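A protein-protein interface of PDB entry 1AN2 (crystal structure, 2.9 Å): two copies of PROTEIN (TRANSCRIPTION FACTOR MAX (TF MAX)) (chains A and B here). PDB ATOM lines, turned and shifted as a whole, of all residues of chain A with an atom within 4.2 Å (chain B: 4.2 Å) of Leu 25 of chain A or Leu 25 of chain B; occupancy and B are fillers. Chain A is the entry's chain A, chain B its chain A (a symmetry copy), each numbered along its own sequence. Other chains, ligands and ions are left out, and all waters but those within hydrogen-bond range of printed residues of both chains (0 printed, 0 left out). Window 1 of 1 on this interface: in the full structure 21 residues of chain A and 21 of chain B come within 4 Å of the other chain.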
ATOM      1  N   SER A  21      17.964  -3.061 -28.741  1.00  0.00           N
ATOM      2  CA  SER A  21      17.928  -3.102 -27.276  1.00  0.00           C
ATOM      3  C   SER A  21      16.772  -3.964 -26.681  1.00  0.00           C
ATOM      4  O   SER A  21      16.696  -4.183 -25.451  1.00  0.00           O
ATOM      5  CB  SER A  21      18.050  -1.680 -26.657  1.00  0.00           C
ATOM      6  OG  SER A  21      19.344  -1.057 -26.917  1.00  0.00           O
ATOM      7  N   PHE A  22      15.992  -4.607 -27.562  1.00  0.00           N
ATOM      8  CA  PHE A  22      14.899  -5.483 -27.108  1.00  0.00           C
ATOM      9  C   PHE A  22      15.375  -6.875 -26.882  1.00  0.00           C
ATOM     10  O   PHE A  22      15.025  -7.473 -25.868  1.00  0.00           O
ATOM     11  CB  PHE A  22      13.718  -5.548 -28.065  1.00  0.00           C
ATOM     12  CG  PHE A  22      12.395  -5.362 -27.375  1.00  0.00           C
ATOM     13  CD1 PHE A  22      11.747  -6.424 -26.813  1.00  0.00           C
ATOM     14  CD2 PHE A  22      11.846  -4.091 -27.228  1.00  0.00           C
ATOM     15  CE1 PHE A  22      10.573  -6.216 -26.106  1.00  0.00           C
ATOM     16  CE2 PHE A  22      10.675  -3.883 -26.523  1.00  0.00           C
ATOM     17  CZ  PHE A  22      10.038  -4.938 -25.960  1.00  0.00           C
ATOM     18  N   HIS A  23      16.122  -7.424 -27.844  1.00  0.00           N
ATOM     19  CA  HIS A  23      16.676  -8.772 -27.666  1.00  0.00           C
ATOM     20  C   HIS A  23      17.668  -8.720 -26.493  1.00  0.00           C
ATOM     21  O   HIS A  23      17.877  -9.711 -25.793  1.00  0.00           O
ATOM     22  CB  HIS A  23      17.382  -9.251 -28.911  1.00  0.00           C
ATOM     23  CG  HIS A  23      18.639  -8.516 -29.196  1.00  0.00           C
ATOM     24  ND1 HIS A  23      18.720  -7.530 -30.156  1.00  0.00           N
ATOM     25  CD2 HIS A  23      19.864  -8.592 -28.624  1.00  0.00           C
ATOM     26  CE1 HIS A  23      19.942  -7.026 -30.162  1.00  0.00           C
ATOM     27  NE2 HIS A  23      20.656  -7.650 -29.240  1.00  0.00           N
ATOM     28  N   SER A  24      18.276  -7.552 -26.295  1.00  0.00           N
ATOM     29  CA  SER A  24      19.190  -7.341 -25.185  1.00  0.00           C
ATOM     30  C   SER A  24      18.377  -7.688 -23.942  1.00  0.00           C
ATOM     31  O   SER A  24      18.929  -8.305 -23.029  1.00  0.00           O
ATOM     32  CB  SER A  24      19.742  -5.900 -25.159  1.00  0.00           C
ATOM     33  OG  SER A  24      20.478  -5.568 -26.364  1.00  0.00           O
ATOM     34  N   LEU A  25      17.069  -7.359 -23.925  1.00  0.00           N
ATOM     35  CA  LEU A  25      16.221  -7.774 -22.771  1.00  0.00           C
ATOM     36  C   LEU A  25      15.944  -9.284 -22.829  1.00  0.00           C
ATOM     37  O   LEU A  25      16.314  -9.999 -21.908  1.00  0.00           O
ATOM     38  CB  LEU A  25      14.867  -7.062 -22.693  1.00  0.00           C
ATOM     39  CG  LEU A  25      14.283  -6.851 -21.270  1.00  0.00           C
ATOM     40  CD1 LEU A  25      12.753  -6.844 -21.202  1.00  0.00           C
ATOM     41  CD2 LEU A  25      14.757  -7.893 -20.330  1.00  0.00           C
ATOM     42  N   ARG A  26      15.283  -9.772 -23.887  1.00  0.00           N
ATOM     43  CA  ARG A  26      14.966 -11.224 -24.033  1.00  0.00           C
ATOM     44  C   ARG A  26      16.113 -12.218 -23.730  1.00  0.00           C
ATOM     45  O   ARG A  26      15.996 -13.044 -22.818  1.00  0.00           O
ATOM     46  CB  ARG A  26      14.439 -11.543 -25.438  1.00  0.00           C
ATOM     47  CG  ARG A  26      14.471 -13.033 -25.786  1.00  0.00           C
ATOM     48  CD  ARG A  26      13.919 -13.259 -27.162  1.00  0.00           C
ATOM     49  NE  ARG A  26      14.970 -13.372 -28.172  1.00  0.00           N
ATOM     50  CZ  ARG A  26      15.090 -12.584 -29.239  1.00  0.00           C
ATOM     51  NH1 ARG A  26      14.237 -11.596 -29.446  1.00  0.00           N
ATOM     52  NH2 ARG A  26      16.011 -12.840 -30.160  1.00  0.00           N
ATOM     53  N   ASP A  27      17.170 -12.179 -24.555  1.00  0.00           N
ATOM     54  CA  ASP A  27      18.335 -13.044 -24.385  1.00  0.00           C
ATOM     55  C   ASP A  27      18.839 -12.802 -22.959  1.00  0.00           C
ATOM     56  O   ASP A  27      19.376 -13.707 -22.325  1.00  0.00           O
ATOM     57  CB  ASP A  27      19.423 -12.759 -25.453  1.00  0.00           C
ATOM     58  CG  ASP A  27      19.093 -13.373 -26.881  1.00  0.00           C
ATOM     59  OD1 ASP A  27      18.014 -13.957 -27.137  1.00  0.00           O
ATOM     60  OD2 ASP A  27      19.940 -13.266 -27.785  1.00  0.00           O
ATOM     61  N   SER A  28      18.571 -11.619 -22.404  1.00  0.00           N
ATOM     62  CA  SER A  28      18.977 -11.359 -21.022  1.00  0.00           C
ATOM     63  C   SER A  28      18.085 -12.167 -20.071  1.00  0.00           C
ATOM     64  O   SER A  28      17.845 -11.776 -18.917  1.00  0.00           O
ATOM     65  CB  SER A  28      18.919  -9.848 -20.712  1.00  0.00           C
ATOM     66  OG  SER A  28      18.530  -9.546 -19.385  1.00  0.00           O
ATOM     67  N   VAL A  29      17.520 -13.258 -20.580  1.00  0.00           N
ATOM     68  CA  VAL A  29      16.682 -14.124 -19.758  1.00  0.00           C
ATOM     69  C   VAL A  29      16.657 -15.529 -20.317  1.00  0.00           C
ATOM     70  O   VAL A  29      16.788 -15.743 -21.528  1.00  0.00           O
ATOM     71  CB  VAL A  29      15.182 -13.684 -19.648  1.00  0.00           C
ATOM     72  CG1 VAL A  29      15.023 -12.171 -19.768  1.00  0.00           C
ATOM     73  CG2 VAL A  29      14.322 -14.421 -20.666  1.00  0.00           C
ATOM     74  N   ILE A  42       8.302 -10.792 -24.062  1.00  0.00           N
ATOM     75  CA  ILE A  42       9.677 -10.562 -23.636  1.00  0.00           C
ATOM     76  C   ILE A  42       9.453  -9.647 -22.426  1.00  0.00           C
ATOM     77  O   ILE A  42      10.295  -9.526 -21.552  1.00  0.00           O
ATOM     78  CB  ILE A  42      10.442  -9.754 -24.713  1.00  0.00           C
ATOM     79  CG1 ILE A  42      10.253 -10.408 -26.088  1.00  0.00           C
ATOM     80  CG2 ILE A  42      11.901  -9.553 -24.310  1.00  0.00           C
ATOM     81  CD1 ILE A  42      11.167  -9.911 -27.205  1.00  0.00           C
ATOM     82  N   ALA A  46      10.086 -11.734 -18.645  1.00  0.00           N
ATOM     83  CA  ALA A  46      11.030 -11.028 -17.802  1.00  0.00           C
ATOM     84  C   ALA A  46      10.334 -10.262 -16.674  1.00  0.00           C
ATOM     85  O   ALA A  46      10.857 -10.213 -15.560  1.00  0.00           O
ATOM     86  CB  ALA A  46      11.935 -10.127 -18.620  1.00  0.00           C
ATOM     87  N   THR A  47       9.105  -9.793 -16.880  1.00  0.00           N
ATOM     88  CA  THR A  47       8.476  -9.031 -15.805  1.00  0.00           C
ATOM     89  C   THR A  47       8.270  -9.883 -14.579  1.00  0.00           C
ATOM     90  O   THR A  47       8.228  -9.386 -13.448  1.00  0.00           O
ATOM     91  CB  THR A  47       7.197  -8.313 -16.219  1.00  0.00           C
ATOM     92  OG1 THR A  47       7.065  -7.129 -15.419  1.00  0.00           O
ATOM     93  CG2 THR A  47       5.974  -9.203 -16.040  1.00  0.00           C
ATOM     94  N   SER B  21       1.572  -3.450 -19.990  1.00  0.00           N
ATOM     95  CA  SER B  21       2.603  -4.429 -19.635  1.00  0.00           C
ATOM     96  C   SER B  21       4.062  -3.877 -19.677  1.00  0.00           C
ATOM     97  O   SER B  21       5.026  -4.570 -19.283  1.00  0.00           O
ATOM     98  CB  SER B  21       2.405  -5.774 -20.393  1.00  0.00           C
ATOM     99  OG  SER B  21       1.178  -6.465 -20.010  1.00  0.00           O
ATOM    100  N   PHE B  22       4.199  -2.576 -19.970  1.00  0.00           N
ATOM    101  CA  PHE B  22       5.528  -1.941 -19.994  1.00  0.00           C
ATOM    102  C   PHE B  22       5.911  -1.429 -18.650  1.00  0.00           C
ATOM    103  O   PHE B  22       7.046  -1.637 -18.229  1.00  0.00           O
ATOM    104  CB  PHE B  22       5.646  -0.787 -20.979  1.00  0.00           C
ATOM    105  CG  PHE B  22       6.876  -0.877 -21.840  1.00  0.00           C
ATOM    106  CD1 PHE B  22       8.068  -0.374 -21.407  1.00  0.00           C
ATOM    107  CD2 PHE B  22       6.837  -1.547 -23.060  1.00  0.00           C
ATOM    108  CE1 PHE B  22       9.207  -0.545 -22.178  1.00  0.00           C
ATOM    109  CE2 PHE B  22       7.973  -1.718 -23.830  1.00  0.00           C
ATOM    110  CZ  PHE B  22       9.156  -1.223 -23.394  1.00  0.00           C
ATOM    111  N   HIS B  23       4.997  -0.711 -17.992  1.00  0.00           N
ATOM    112  CA  HIS B  23       5.282  -0.222 -16.637  1.00  0.00           C
ATOM    113  C   HIS B  23       5.434  -1.446 -15.719  1.00  0.00           C
ATOM    114  O   HIS B  23       6.155  -1.408 -14.722  1.00  0.00           O
ATOM    115  CB  HIS B  23       4.176   0.667 -16.123  1.00  0.00           C
ATOM    116  CG  HIS B  23       2.913  -0.062 -15.850  1.00  0.00           C
ATOM    117  ND1 HIS B  23       1.836  -0.027 -16.709  1.00  0.00           N
ATOM    118  CD2 HIS B  23       2.559  -0.878 -14.830  1.00  0.00           C
ATOM    119  CE1 HIS B  23       0.871  -0.795 -16.233  1.00  0.00           C
ATOM    120  NE2 HIS B  23       1.285  -1.326 -15.094  1.00  0.00           N
ATOM    121  N   SER B  24       4.742  -2.528 -16.072  1.00  0.00           N
ATOM    122  CA  SER B  24       4.839  -3.775 -15.333  1.00  0.00           C
ATOM    123  C   SER B  24       6.325  -4.119 -15.346  1.00  0.00           C
ATOM    124  O   SER B  24       6.832  -4.586 -14.324  1.00  0.00           O
ATOM    125  CB  SER B  24       3.962  -4.883 -15.954  1.00  0.00           C
ATOM    126  OG  SER B  24       2.556  -4.528 -15.974  1.00  0.00           O
ATOM    127  N   LEU B  25       7.035  -3.833 -16.457  1.00  0.00           N
ATOM    128  CA  LEU B  25       8.509  -4.060 -16.467  1.00  0.00           C
ATOM    129  C   LEU B  25       9.217  -2.992 -15.620  1.00  0.00           C
ATOM    130  O   LEU B  25       9.881  -3.337 -14.652  1.00  0.00           O
ATOM    131  CB  LEU B  25       9.142  -4.034 -17.862  1.00  0.00           C
ATOM    132  CG  LEU B  25      10.395  -4.929 -18.064  1.00  0.00           C
ATOM    133  CD1 LEU B  25      11.400  -4.399 -19.090  1.00  0.00           C
ATOM    134  CD2 LEU B  25      11.129  -5.127 -16.794  1.00  0.00           C
ATOM    135  N   ARG B  26       9.101  -1.709 -15.983  1.00  0.00           N
ATOM    136  CA  ARG B  26       9.754  -0.600 -15.223  1.00  0.00           C
ATOM    137  C   ARG B  26       9.616  -0.640 -13.682  1.00  0.00           C
ATOM    138  O   ARG B  26      10.622  -0.726 -12.969  1.00  0.00           O
ATOM    139  CB  ARG B  26       9.253   0.771 -15.695  1.00  0.00           C
ATOM    140  CG  ARG B  26       9.564   1.911 -14.721  1.00  0.00           C
ATOM    141  CD  ARG B  26       9.065   3.214 -15.267  1.00  0.00           C
ATOM    142  NE  ARG B  26       7.761   3.586 -14.718  1.00  0.00           N
ATOM    143  CZ  ARG B  26       6.663   3.800 -15.440  1.00  0.00           C
ATOM    144  NH1 ARG B  26       6.684   3.666 -16.754  1.00  0.00           N
ATOM    145  NH2 ARG B  26       5.556   4.246 -14.857  1.00  0.00           N
ATOM    146  N   ASP B  27       8.377  -0.493 -13.190  1.00  0.00           N
ATOM    147  CA  ASP B  27       8.088  -0.526 -11.758  1.00  0.00           C
ATOM    148  C   ASP B  27       8.646  -1.856 -11.243  1.00  0.00           C
ATOM    149  O   ASP B  27       9.083  -1.949 -10.098  1.00  0.00           O
ATOM    150  CB  ASP B  27       6.571  -0.371 -11.474  1.00  0.00           C
ATOM    151  CG  ASP B  27       6.044   1.121 -11.612  1.00  0.00           C
ATOM    152  OD1 ASP B  27       6.771   2.066 -12.000  1.00  0.00           O
ATOM    153  OD2 ASP B  27       4.857   1.362 -11.329  1.00  0.00           O
ATOM    154  N   SER B  28       8.741  -2.863 -12.115  1.00  0.00           N
ATOM    155  CA  SER B  28       9.324  -4.136 -11.689  1.00  0.00           C
ATOM    156  C   SER B  28      10.837  -3.964 -11.505  1.00  0.00           C
ATOM    157  O   SER B  28      11.622  -4.913 -11.663  1.00  0.00           O
ATOM    158  CB  SER B  28       8.996  -5.251 -12.704  1.00  0.00           C
ATOM    159  OG  SER B  28      10.026  -6.210 -12.860  1.00  0.00           O
ATOM    160  N   VAL B  29      11.262  -2.729 -11.252  1.00  0.00           N
ATOM    161  CA  VAL B  29      12.676  -2.454 -11.022  1.00  0.00           C
ATOM    162  C   VAL B  29      12.847  -1.198 -10.196  1.00  0.00           C
ATOM    163  O   VAL B  29      12.025  -0.276 -10.247  1.00  0.00           O
ATOM    164  CB  VAL B  29      13.527  -2.228 -12.318  1.00  0.00           C
ATOM    165  CG1 VAL B  29      12.970  -3.008 -13.506  1.00  0.00           C
ATOM    166  CG2 VAL B  29      13.658  -0.744 -12.632  1.00  0.00           C
ATOM    167  N   ILE B  42      13.762   1.690 -20.049  1.00  0.00           N
ATOM    168  CA  ILE B  42      13.098   0.731 -19.174  1.00  0.00           C
ATOM    169  C   ILE B  42      13.712  -0.583 -19.673  1.00  0.00           C
ATOM    170  O   ILE B  42      13.728  -1.585 -18.977  1.00  0.00           O
ATOM    171  CB  ILE B  42      11.579   0.695 -19.475  1.00  0.00           C
ATOM    172  CG1 ILE B  42      11.014   2.122 -19.478  1.00  0.00           C
ATOM    173  CG2 ILE B  42      10.858  -0.262 -18.529  1.00  0.00           C
ATOM    174  CD1 ILE B  42       9.493   2.248 -19.470  1.00  0.00           C
ATOM    175  N   ALA B  46      16.670  -2.177 -16.888  1.00  0.00           N
ATOM    176  CA  ALA B  46      16.381  -3.553 -16.537  1.00  0.00           C
ATOM    177  C   ALA B  46      17.291  -4.540 -17.272  1.00  0.00           C
ATOM    178  O   ALA B  46      17.699  -5.543 -16.685  1.00  0.00           O
ATOM    179  CB  ALA B  46      14.914  -3.879 -16.745  1.00  0.00           C
ATOM    180  N   THR B  47      17.746  -4.216 -18.480  1.00  0.00           N
ATOM    181  CA  THR B  47      18.581  -5.189 -19.180  1.00  0.00           C
ATOM    182  C   THR B  47      19.866  -5.443 -18.434  1.00  0.00           C
ATOM    183  O   THR B  47      20.471  -6.516 -18.537  1.00  0.00           O
ATOM    184  CB  THR B  47      18.832  -4.852 -20.645  1.00  0.00           C
ATOM    185  OG1 THR B  47      19.007  -6.081 -21.366  1.00  0.00           O
ATOM    186  CG2 THR B  47      20.060  -3.969 -20.813  1.00  0.00           C
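N of Leu 25 of chain A is in hydrogen-bond range of OG1 of Thr 47 of chain B, 3.5 Å away.
The backbone carbonyl oxygen of Ser 24 of chain A is in hydrogen-bond range of the side-chain hydroxyl of Thr 47 of chain B.
The backbone NH (N) of Leu 25 of chain B is in hydrogen-bond range of the side-chain hydroxyl (OG1) of Thr 47 of chain A, 3.5 Å away.
The backbone carbonyl oxygen of Ser 24 of chain B is in hydrogen-bond range of the side-chain hydroxyl of Thr 47 of chain A, at 2.8 Å.
Hydrophobic or aromatic side chains of chain A that line the printed part of chain B: Leu 25.
Of the 12 printed residues of chain B, 4 touch a printed residue of chain A.
Among the printed residues, no Asp or Glu carboxylate lies within 4 Å of a Lys or Arg side-chain nitrogen of the other chain.
Ser 24 of chain A touches Thr 47 of chain B, and with the chains exchanged Thr 47 of chain A touches Ser 24 of chain B.
Leu 25 of chain A touches its own counterpart, Leu 25 of chain B.
Leu 25 of chain A touches Thr 47 of chain B, and with the chains exchanged Thr 47 of chain A touches Leu 25 of chain B.
Ser 28 of chain A touches Thr 47 of chain B, and with the chains exchanged Thr 47 of chain A touches Ser 28 of chain B.
12 positions are printed for both chains.
Of the 7 pairs that touch across the chains among the printed residues, 7 have their exchanged pair printed and touching as well.
The backbone carbonyl oxygen of Leu 25 of chain A sits close to the side-chain hydroxyl of Ser 28 of chain A (3.4 Å).
The side-chain hydroxyl (OG) of Ser 28 of chain B lies close to the backbone carbonyl oxygen (O) of Leu 25 of chain B (3.4 Å).
Leu 25 of chain A touches just these residues of chain B: Leu 25 (3.5 Å) and Thr 47 (3.5 Å).
Leu 25 of chain B touches two residues of chain A.
Printed residues of chain B within 4 Å of Ser 28 of chain A: Thr 47.
Of the printed residues of chain B, Ser 24 of chain A touches Thr 47.
Printed residues of chain A within 4 Å of Thr 47 of chain B: Ser 24, Leu 25 and Ser 28.
Printed residues of chain A within 4 Å of Ser 28 of chain B: Thr 47 (3.7 Å).
The nearest printed residue of chain B that does not touch Leu 25 of chain A is Ala 46 of chain B (5.2 Å).
The nearest printed residue of chain A that does not touch Leu 25 of chain B is Ala 46 of chain A (5.2 Å).
The nearest printed residue of chain A that does not touch Ser 28 of chain B is Ala 46 of chain A (4.9 Å).
Leu 25 of chain A touches Leu 25 of chain B.
OG of Ser 28 of chain A touches O of Thr 47 of chain B, 3.7 Å away.
O of Thr 47 of chain A touches OG of Ser 28 of chain B, 3.7 Å away.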
